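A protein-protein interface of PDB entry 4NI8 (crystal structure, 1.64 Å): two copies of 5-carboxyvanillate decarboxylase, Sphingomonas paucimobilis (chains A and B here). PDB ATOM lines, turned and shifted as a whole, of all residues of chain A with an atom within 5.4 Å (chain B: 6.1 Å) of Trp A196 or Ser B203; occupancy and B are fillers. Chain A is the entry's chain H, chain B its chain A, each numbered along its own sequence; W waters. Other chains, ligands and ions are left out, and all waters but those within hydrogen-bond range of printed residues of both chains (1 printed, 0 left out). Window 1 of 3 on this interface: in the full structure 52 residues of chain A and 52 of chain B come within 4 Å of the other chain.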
ATOM      1  N   PHE A 186      19.691 -27.464  18.084  1.00  0.00           N
ATOM      2  CA  PHE A 186      18.424 -26.890  17.636  1.00  0.00           C
ATOM      3  C   PHE A 186      17.274 -27.211  18.581  1.00  0.00           C
ATOM      4  O   PHE A 186      16.109 -27.224  18.176  1.00  0.00           O
ATOM      5  CB  PHE A 186      18.113 -27.366  16.217  1.00  0.00           C
ATOM      6  CG  PHE A 186      19.179 -26.992  15.223  1.00  0.00           C
ATOM      7  CD1 PHE A 186      20.301 -27.786  15.060  1.00  0.00           C
ATOM      8  CD2 PHE A 186      19.094 -25.813  14.513  1.00  0.00           C
ATOM      9  CE1 PHE A 186      21.309 -27.425  14.169  1.00  0.00           C
ATOM     10  CE2 PHE A 186      20.091 -25.448  13.618  1.00  0.00           C
ATOM     11  CZ  PHE A 186      21.196 -26.258  13.448  1.00  0.00           C
ATOM     12  N   MET A 191      14.154 -23.380  17.617  1.00  0.00           N
ATOM     13  CA  MET A 191      15.042 -23.478  16.460  1.00  0.00           C
ATOM     14  C   MET A 191      14.961 -24.818  15.709  1.00  0.00           C
ATOM     15  O   MET A 191      15.602 -24.980  14.681  1.00  0.00           O
ATOM     16  CB  MET A 191      16.484 -23.164  16.851  1.00  0.00           C
ATOM     17  CG  MET A 191      16.655 -21.725  17.316  1.00  0.00           C
ATOM     18  SD  MET A 191      18.279 -21.363  17.979  1.00  0.00           S
ATOM     19  CE  MET A 191      19.366 -21.753  16.602  1.00  0.00           C
ATOM     20  N   SER A 193      12.554 -25.615  14.040  1.00  0.00           N
ATOM     21  CA  SER A 193      11.578 -25.391  12.984  1.00  0.00           C
ATOM     22  C   SER A 193      12.066 -24.421  11.905  1.00  0.00           C
ATOM     23  O   SER A 193      13.265 -24.275  11.657  1.00  0.00           O
ATOM     24  CB  SER A 193      10.270 -24.880  13.619  1.00  0.00           C
ATOM     25  OG  SER A 193       9.208 -24.806  12.684  1.00  0.00           O
ATOM     26  N   ALA A 194      11.106 -23.762  11.274  1.00  0.00           N
ATOM     27  CA  ALA A 194      11.356 -22.873  10.147  1.00  0.00           C
ATOM     28  C   ALA A 194      12.269 -21.689  10.482  1.00  0.00           C
ATOM     29  O   ALA A 194      12.961 -21.165   9.604  1.00  0.00           O
ATOM     30  CB  ALA A 194      10.032 -22.385   9.567  1.00  0.00           C
ATOM     31  N   ILE A 195      12.308 -21.293  11.749  1.00  0.00           N
ATOM     32  CA  ILE A 195      13.053 -20.092  12.119  1.00  0.00           C
ATOM     33  C   ILE A 195      14.567 -20.263  11.913  1.00  0.00           C
ATOM     34  O   ILE A 195      15.278 -19.286  11.725  1.00  0.00           O
ATOM     35  CB  ILE A 195      12.738 -19.623  13.560  1.00  0.00           C
ATOM     36  CG1 ILE A 195      13.190 -18.167  13.765  1.00  0.00           C
ATOM     37  CG2 ILE A 195      13.356 -20.570  14.608  1.00  0.00           C
ATOM     38  CD1 ILE A 195      12.687 -17.545  15.079  1.00  0.00           C
ATOM     39  N   TRP A 196      15.060 -21.498  11.943  1.00  0.00           N
ATOM     40  CA  TRP A 196      16.493 -21.707  11.731  1.00  0.00           C
ATOM     41  C   TRP A 196      16.860 -23.140  11.326  1.00  0.00           C
ATOM     42  O   TRP A 196      17.512 -23.343  10.308  1.00  0.00           O
ATOM     43  CB  TRP A 196      17.315 -21.229  12.953  1.00  0.00           C
ATOM     44  CG  TRP A 196      18.767 -21.108  12.639  1.00  0.00           C
ATOM     45  CD1 TRP A 196      19.784 -21.866  13.145  1.00  0.00           C
ATOM     46  CD2 TRP A 196      19.366 -20.200  11.704  1.00  0.00           C
ATOM     47  NE1 TRP A 196      20.988 -21.475  12.588  1.00  0.00           N
ATOM     48  CE2 TRP A 196      20.752 -20.467  11.690  1.00  0.00           C
ATOM     49  CE3 TRP A 196      18.860 -19.197  10.870  1.00  0.00           C
ATOM     50  CZ2 TRP A 196      21.643 -19.751  10.887  1.00  0.00           C
ATOM     51  CZ3 TRP A 196      19.738 -18.493  10.070  1.00  0.00           C
ATOM     52  CH2 TRP A 196      21.116 -18.773  10.080  1.00  0.00           C
ATOM     53  N   GLY A 197      16.439 -24.120  12.115  1.00  0.00           N
ATOM     54  CA  GLY A 197      16.768 -25.513  11.837  1.00  0.00           C
ATOM     55  C   GLY A 197      16.450 -26.017  10.430  1.00  0.00           C
ATOM     56  O   GLY A 197      17.258 -26.729   9.820  1.00  0.00           O
ATOM     57  N   TYR A 198      15.270 -25.663   9.920  1.00  0.00           N
ATOM     58  CA  TYR A 198      14.847 -26.109   8.594  1.00  0.00           C
ATOM     59  C   TYR A 198      15.874 -25.721   7.527  1.00  0.00           C
ATOM     60  O   TYR A 198      16.252 -26.531   6.677  1.00  0.00           O
ATOM     61  CB  TYR A 198      13.479 -25.521   8.241  1.00  0.00           C
ATOM     62  CG  TYR A 198      12.300 -26.289   8.810  1.00  0.00           C
ATOM     63  CD1 TYR A 198      12.491 -27.316   9.734  1.00  0.00           C
ATOM     64  CD2 TYR A 198      11.001 -25.986   8.421  1.00  0.00           C
ATOM     65  CE1 TYR A 198      11.404 -28.022  10.258  1.00  0.00           C
ATOM     66  CE2 TYR A 198       9.904 -26.690   8.932  1.00  0.00           C
ATOM     67  CZ  TYR A 198      10.119 -27.706   9.845  1.00  0.00           C
ATOM     68  OH  TYR A 198       9.046 -28.401  10.351  1.00  0.00           O
ATOM     69  N   GLY A 199      16.327 -24.475   7.579  1.00  0.00           N
ATOM     70  CA  GLY A 199      17.265 -23.987   6.575  1.00  0.00           C
ATOM     71  C   GLY A 199      18.653 -24.610   6.667  1.00  0.00           C
ATOM     72  O   GLY A 199      19.294 -24.876   5.647  1.00  0.00           O
ATOM     73  N   ILE A 200      19.129 -24.825   7.891  1.00  0.00           N
ATOM     74  CA  ILE A 200      20.442 -25.428   8.102  1.00  0.00           C
ATOM     75  C   ILE A 200      20.451 -26.892   7.666  1.00  0.00           C
ATOM     76  O   ILE A 200      21.391 -27.363   7.025  1.00  0.00           O
ATOM     77  CB  ILE A 200      20.861 -25.318   9.590  1.00  0.00           C
ATOM     78  CG1 ILE A 200      20.871 -23.848  10.015  1.00  0.00           C
ATOM     79  CG2 ILE A 200      22.226 -25.980   9.818  1.00  0.00           C
ATOM     80  CD1 ILE A 200      21.800 -22.965   9.187  1.00  0.00           C
ATOM     81  N   GLU A 201      19.387 -27.603   8.016  1.00  0.00           N
ATOM     82  CA  GLU A 201      19.241 -29.011   7.658  1.00  0.00           C
ATOM     83  C   GLU A 201      19.205 -29.184   6.132  1.00  0.00           C
ATOM     84  O   GLU A 201      19.949 -29.997   5.562  1.00  0.00           O
ATOM     85  CB  GLU A 201      17.969 -29.551   8.325  1.00  0.00           C
ATOM     86  CG  GLU A 201      17.361 -30.800   7.714  1.00  0.00           C
ATOM     87  CD  GLU A 201      18.223 -32.031   7.844  1.00  0.00           C
ATOM     88  OE1 GLU A 201      19.119 -32.073   8.720  1.00  0.00           O
ATOM     89  OE2 GLU A 201      17.986 -32.972   7.053  1.00  0.00           O
ATOM     90  N   SER B 145      33.946 -18.688  17.538  1.00  0.00           N
ATOM     91  CA  SER B 145      32.667 -19.325  17.850  1.00  0.00           C
ATOM     92  C   SER B 145      32.652 -20.056  19.200  1.00  0.00           C
ATOM     93  O   SER B 145      33.000 -19.458  20.206  1.00  0.00           O
ATOM     94  CB  SER B 145      32.162 -20.187  16.689  1.00  0.00           C
ATOM     95  OG  SER B 145      30.756 -20.392  16.803  1.00  0.00           O
ATOM     96  N   TYR B 198      32.341 -23.700   8.894  1.00  0.00           N
ATOM     97  CA  TYR B 198      32.602 -22.431   9.585  1.00  0.00           C
ATOM     98  C   TYR B 198      31.369 -21.540   9.623  1.00  0.00           C
ATOM     99  O   TYR B 198      31.028 -20.978  10.662  1.00  0.00           O
ATOM    100  CB  TYR B 198      33.750 -21.654   8.922  1.00  0.00           C
ATOM    101  CG  TYR B 198      35.143 -22.128   9.288  1.00  0.00           C
ATOM    102  CD1 TYR B 198      35.341 -23.300  10.023  1.00  0.00           C
ATOM    103  CD2 TYR B 198      36.263 -21.397   8.904  1.00  0.00           C
ATOM    104  CE1 TYR B 198      36.625 -23.734  10.358  1.00  0.00           C
ATOM    105  CE2 TYR B 198      37.540 -21.816   9.243  1.00  0.00           C
ATOM    106  CZ  TYR B 198      37.715 -22.983   9.961  1.00  0.00           C
ATOM    107  OH  TYR B 198      38.997 -23.399  10.285  1.00  0.00           O
ATOM    108  N   GLY B 199      30.704 -21.407   8.480  1.00  0.00           N
ATOM    109  CA  GLY B 199      29.529 -20.555   8.396  1.00  0.00           C
ATOM    110  C   GLY B 199      28.329 -21.043   9.187  1.00  0.00           C
ATOM    111  O   GLY B 199      27.603 -20.246   9.767  1.00  0.00           O
ATOM    112  N   ILE B 200      28.101 -22.355   9.190  1.00  0.00           N
ATOM    113  CA  ILE B 200      26.964 -22.927   9.904  1.00  0.00           C
ATOM    114  C   ILE B 200      27.183 -22.847  11.414  1.00  0.00           C
ATOM    115  O   ILE B 200      26.269 -22.524  12.178  1.00  0.00           O
ATOM    116  CB  ILE B 200      26.757 -24.411   9.504  1.00  0.00           C
ATOM    117  CG1 ILE B 200      26.495 -24.527   7.999  1.00  0.00           C
ATOM    118  CG2 ILE B 200      25.641 -25.036  10.342  1.00  0.00           C
ATOM    119  CD1 ILE B 200      25.326 -23.671   7.501  1.00  0.00           C
ATOM    120  N   GLU B 201      28.407 -23.147  11.839  1.00  0.00           N
ATOM    121  CA  GLU B 201      28.784 -23.080  13.254  1.00  0.00           C
ATOM    122  C   GLU B 201      28.621 -21.659  13.810  1.00  0.00           C
ATOM    123  O   GLU B 201      28.004 -21.446  14.863  1.00  0.00           O
ATOM    124  CB  GLU B 201      30.241 -23.552  13.406  1.00  0.00           C
ATOM    125  CG  GLU B 201      30.974 -23.088  14.665  1.00  0.00           C
ATOM    126  CD  GLU B 201      30.422 -23.665  15.954  1.00  0.00           C
ATOM    127  OE1 GLU B 201      29.758 -24.731  15.936  1.00  0.00           O
ATOM    128  OE2 GLU B 201      30.673 -23.045  17.005  1.00  0.00           O
ATOM    129  N   THR B 202      29.158 -20.694  13.083  1.00  0.00           N
ATOM    130  CA  THR B 202      29.210 -19.311  13.565  1.00  0.00           C
ATOM    131  C   THR B 202      27.835 -18.618  13.512  1.00  0.00           C
ATOM    132  O   THR B 202      27.449 -17.919  14.456  1.00  0.00           O
ATOM    133  CB  THR B 202      30.246 -18.498  12.781  1.00  0.00           C
ATOM    134  OG1 THR B 202      31.490 -19.223  12.761  1.00  0.00           O
ATOM    135  CG2 THR B 202      30.466 -17.138  13.432  1.00  0.00           C
ATOM    136  N   SER B 203      27.091 -18.831  12.425  1.00  0.00           N
ATOM    137  CA  SER B 203      25.754 -18.258  12.304  1.00  0.00           C
ATOM    138  C   SER B 203      24.803 -18.845  13.341  1.00  0.00           C
ATOM    139  O   SER B 203      23.971 -18.136  13.882  1.00  0.00           O
ATOM    140  CB  SER B 203      25.178 -18.446  10.895  1.00  0.00           C
ATOM    141  OG  SER B 203      25.056 -19.826  10.546  1.00  0.00           O
ATOM    142  N   THR B 204      24.908 -20.147  13.592  1.00  0.00           N
ATOM    143  CA  THR B 204      24.033 -20.777  14.580  1.00  0.00           C
ATOM    144  C   THR B 204      24.327 -20.249  15.978  1.00  0.00           C
ATOM    145  O   THR B 204      23.407 -20.011  16.761  1.00  0.00           O
ATOM    146  CB  THR B 204      24.145 -22.320  14.522  1.00  0.00           C
ATOM    147  OG1 THR B 204      23.749 -22.763  13.214  1.00  0.00           O
ATOM    148  CG2 THR B 204      23.246 -22.985  15.591  1.00  0.00           C
ATOM    149  N   ASN B 205      25.606 -20.049  16.288  1.00  0.00           N
ATOM    150  CA  ASN B 205      25.989 -19.406  17.546  1.00  0.00           C
ATOM    151  C   ASN B 205      25.300 -18.033  17.654  1.00  0.00           C
ATOM    152  O   ASN B 205      24.606 -17.750  18.631  1.00  0.00           O
ATOM    153  CB  ASN B 205      27.516 -19.256  17.622  1.00  0.00           C
ATOM    154  CG  ASN B 205      28.020 -18.979  19.044  1.00  0.00           C
ATOM    155  OD1 ASN B 205      27.245 -18.722  19.966  1.00  0.00           O
ATOM    156  ND2 ASN B 205      29.334 -19.049  19.217  1.00  0.00           N
ATOM    157  N   ALA B 206      25.451 -17.205  16.629  1.00  0.00           N
ATOM    158  CA  ALA B 206      24.888 -15.851  16.662  1.00  0.00           C
ATOM    159  C   ALA B 206      23.352 -15.859  16.742  1.00  0.00           C
ATOM    160  O   ALA B 206      22.757 -15.044  17.452  1.00  0.00           O
ATOM    161  CB  ALA B 206      25.353 -15.036  15.454  1.00  0.00           C
ATOM    162  N   VAL B 207      22.705 -16.769  16.012  1.00  0.00           N
ATOM    163  CA  VAL B 207      21.246 -16.852  16.069  1.00  0.00           C
ATOM    164  C   VAL B 207      20.777 -17.270  17.468  1.00  0.00           C
ATOM    165  O   VAL B 207      19.794 -16.731  17.987  1.00  0.00           O
ATOM    166  CB  VAL B 207      20.675 -17.787  14.958  1.00  0.00           C
ATOM    167  CG1 VAL B 207      19.214 -18.116  15.210  1.00  0.00           C
ATOM    168  CG2 VAL B 207      20.849 -17.140  13.575  1.00  0.00           C
ATOM    169  N   ARG B 208      21.484 -18.212  18.093  1.00  0.00           N
ATOM    170  CA  ARG B 208      21.147 -18.565  19.478  1.00  0.00           C
ATOM    171  C   ARG B 208      21.302 -17.358  20.399  1.00  0.00           C
ATOM    172  O   ARG B 208      20.466 -17.136  21.281  1.00  0.00           O
ATOM    173  CB  ARG B 208      21.998 -19.726  19.997  1.00  0.00           C
ATOM    174  CG  ARG B 208      21.768 -21.058  19.302  1.00  0.00           C
ATOM    175  CD  ARG B 208      22.751 -22.112  19.823  1.00  0.00           C
ATOM    176  NE  ARG B 208      22.506 -22.405  21.233  1.00  0.00           N
ATOM    177  CZ  ARG B 208      21.799 -23.439  21.678  1.00  0.00           C
ATOM    178  NH1 ARG B 208      21.274 -24.313  20.827  1.00  0.00           N
ATOM    179  NH2 ARG B 208      21.620 -23.609  22.984  1.00  0.00           N
ATOM    180  N   LEU B 211      18.150 -15.097  19.725  1.00  0.00           N
ATOM    181  CA  LEU B 211      16.855 -15.646  20.129  1.00  0.00           C
ATOM    182  C   LEU B 211      16.759 -15.903  21.629  1.00  0.00           C
ATOM    183  O   LEU B 211      15.669 -15.945  22.195  1.00  0.00           O
ATOM    184  CB  LEU B 211      16.545 -16.925  19.356  1.00  0.00           C
ATOM    185  CG  LEU B 211      16.441 -16.745  17.842  1.00  0.00           C
ATOM    186  CD1 LEU B 211      16.058 -18.073  17.179  1.00  0.00           C
ATOM    187  CD2 LEU B 211      15.414 -15.677  17.512  1.00  0.00           C
ATOM    188  N   LEU B 225      30.593 -10.060  12.693  1.00  0.00           N
ATOM    189  CA  LEU B 225      30.663 -11.342  11.997  1.00  0.00           C
ATOM    190  C   LEU B 225      31.279 -11.173  10.611  1.00  0.00           C
ATOM    191  O   LEU B 225      30.844 -10.308   9.830  1.00  0.00           O
ATOM    192  CB  LEU B 225      29.259 -11.949  11.848  1.00  0.00           C
ATOM    193  CG  LEU B 225      28.491 -12.303  13.117  1.00  0.00           C
ATOM    194  CD1 LEU B 225      27.089 -12.767  12.734  1.00  0.00           C
ATOM    195  CD2 LEU B 225      29.236 -13.399  13.865  1.00  0.00           C
ATOM    196  N   GLY B 229      28.538 -11.597   7.162  1.00  0.00           N
ATOM    197  CA  GLY B 229      27.588 -11.824   8.243  1.00  0.00           C
ATOM    198  C   GLY B 229      27.193 -13.283   8.427  1.00  0.00           C
ATOM    199  O   GLY B 229      26.156 -13.587   9.038  1.00  0.00           O
ATOM    200  N   GLU B 230      28.027 -14.186   7.917  1.00  0.00           N
ATOM    201  CA  GLU B 230      27.752 -15.621   7.971  1.00  0.00           C
ATOM    202  C   GLU B 230      26.333 -15.909   7.453  1.00  0.00           C
ATOM    203  O   GLU B 230      25.633 -16.796   7.958  1.00  0.00           O
ATOM    204  CB  GLU B 230      27.965 -16.188   9.391  1.00  0.00           C
ATOM    205  CG  GLU B 230      29.302 -15.786  10.052  1.00  0.00           C
ATOM    206  CD  GLU B 230      30.534 -16.426   9.405  1.00  0.00           C
ATOM    207  OE1 GLU B 230      30.386 -17.242   8.471  1.00  0.00           O
ATOM    208  OE2 GLU B 230      31.666 -16.112   9.845  1.00  0.00           O
ATOM    209  N   ALA B 231      25.939 -15.124   6.445  1.00  0.00           N
ATOM    210  CA  ALA B 231      24.659 -15.233   5.727  1.00  0.00           C
ATOM    211  C   ALA B 231      23.430 -14.820   6.521  1.00  0.00           C
ATOM    212  O   ALA B 231      22.334 -14.827   5.975  1.00  0.00           O
ATOM    213  CB  ALA B 231      24.455 -16.630   5.120  1.00  0.00           C
ATOM    214  N   ILE B 232      23.602 -14.453   7.786  1.00  0.00           N
ATOM    215  CA  ILE B 232      22.447 -13.969   8.554  1.00  0.00           C
ATOM    216  C   ILE B 232      21.714 -12.786   7.871  1.00  0.00           C
ATOM    217  O   ILE B 232      20.467 -12.730   7.913  1.00  0.00           O
ATOM    218  CB  ILE B 232      22.809 -13.664  10.025  1.00  0.00           C
ATOM    219  CG1 ILE B 232      23.181 -14.970  10.735  1.00  0.00           C
ATOM    220  CG2 ILE B 232      21.643 -12.978  10.737  1.00  0.00           C
ATOM    221  CD1 ILE B 232      23.721 -14.784  12.117  1.00  0.00           C
ATOM    222  N   TRP B 235      18.879 -14.071   5.789  1.00  0.00           N
ATOM    223  CA  TRP B 235      17.773 -14.753   6.464  1.00  0.00           C
ATOM    224  C   TRP B 235      16.864 -13.822   7.286  1.00  0.00           C
ATOM    225  O   TRP B 235      15.950 -14.302   7.961  1.00  0.00           O
ATOM    226  CB  TRP B 235      18.313 -15.821   7.416  1.00  0.00           C
ATOM    227  CG  TRP B 235      18.918 -17.064   6.803  1.00  0.00           C
ATOM    228  CD1 TRP B 235      20.261 -17.376   6.724  1.00  0.00           C
ATOM    229  CD2 TRP B 235      18.214 -18.193   6.266  1.00  0.00           C
ATOM    230  NE1 TRP B 235      20.419 -18.619   6.156  1.00  0.00           N
ATOM    231  CE2 TRP B 235      19.181 -19.133   5.855  1.00  0.00           C
ATOM    232  CE3 TRP B 235      16.858 -18.482   6.061  1.00  0.00           C
ATOM    233  CZ2 TRP B 235      18.837 -20.351   5.256  1.00  0.00           C
ATOM    234  CZ3 TRP B 235      16.516 -19.699   5.466  1.00  0.00           C
ATOM    235  CH2 TRP B 235      17.504 -20.619   5.080  1.00  0.00           C
ATOM    236  N   LEU B 239      13.701 -14.978   9.724  1.00  0.00           N
ATOM    237  CA  LEU B 239      13.951 -14.908  11.167  1.00  0.00           C
ATOM    238  C   LEU B 239      12.867 -14.093  11.865  1.00  0.00           C
ATOM    239  O   LEU B 239      12.314 -14.516  12.886  1.00  0.00           O
ATOM    240  CB  LEU B 239      15.323 -14.302  11.459  1.00  0.00           C
ATOM    241  CG  LEU B 239      16.524 -15.222  11.225  1.00  0.00           C
ATOM    242  CD1 LEU B 239      17.800 -14.397  11.147  1.00  0.00           C
ATOM    243  CD2 LEU B 239      16.636 -16.279  12.320  1.00  0.00           C
HETATM  244  O   HOH W   1      18.534 -24.343  19.620  1.00  0.00           O
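The side-chain hydroxyl (OG1) of Thr B204 is in hydrogen-bond range of the indole nitrogen (NE1) of Trp A196 (3.1 Å).
The backbone carbonyl oxygen of Gly B199 lies within hydrogen-bond range of the side-chain hydroxyl of Ser B203. OG of Ser B203 is in hydrogen-bond range of O of Ile B200, 3.4 Å away. The backbone carbonyl oxygen (O) of Ile B200 sits at hydrogen-bond distance from the side-chain hydroxyl (OG1) of Thr B204. The backbone carbonyl oxygen (O) of Met A191 lies within hydrogen-bond range of the backbone NH (N) of Gly A197, 2.8 Å away.
Among the printed residues, pairs that only touch across the chains: Met A191 with Val B207 (3.9 Å), Met A191 with Arg B208 (3.7 Å), Met A191 with Leu B211 (3.7 Å), Ile A195 with Leu B239 (3.4 Å), Trp A196 with Ser B203 (3.4 Å), Trp A196 with Val B207 (3.8 Å), Trp A196 with Trp B235 (3.6 Å), Trp A196 with Leu B239 (3.9 Å), Gly A199 with Trp B235 (3.7 Å) and Ile A200 with Ile B200 (3.6 Å).
Trp A196 touches five residues of chain B. Of the printed residues of chain B, Ile A200 touches Ile B200 (3.6 Å). Printed residues of chain A within 4 Å of Ile B200: Ile A200 (3.6 Å). Ser B203 touches just one residue of chain A: Trp A196 (3.4 Å). The nearest residue of chain B that does not touch Trp A196 is Ile B232 (4.4 Å). The nearest residue of chain A that does not touch Ser B203 is Ile A200 (4.7 Å). The nearest printed residue of chain B that does not touch Ile A200 is Thr B204 (4.4 Å).
Hydrophobic or aromatic side chains of chain A within 4 Å of the printed part of chain B: Met A191, Ile A195, Trp A196 and Ile A200. Along chain A the printed residues that touch a printed residue of chain B span positions 191 to 200. Hydrophobic or aromatic side chains of chain B that line the printed part of chain A: Ile B200, Val B207, Leu B211, Trp B235 and Leu B239. Along chain B the printed residues that touch a printed residue of chain A span positions 200 to 239. Among the printed residues, no Asp or Glu carboxylate lies within 4 Å of a Lys or Arg side-chain nitrogen of the other chain.
Ile A200 touches its own counterpart, Ile B200. 4 positions are printed for both chains.
Water W1 bridges NH1 of Arg B208 and SD of Met A191.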
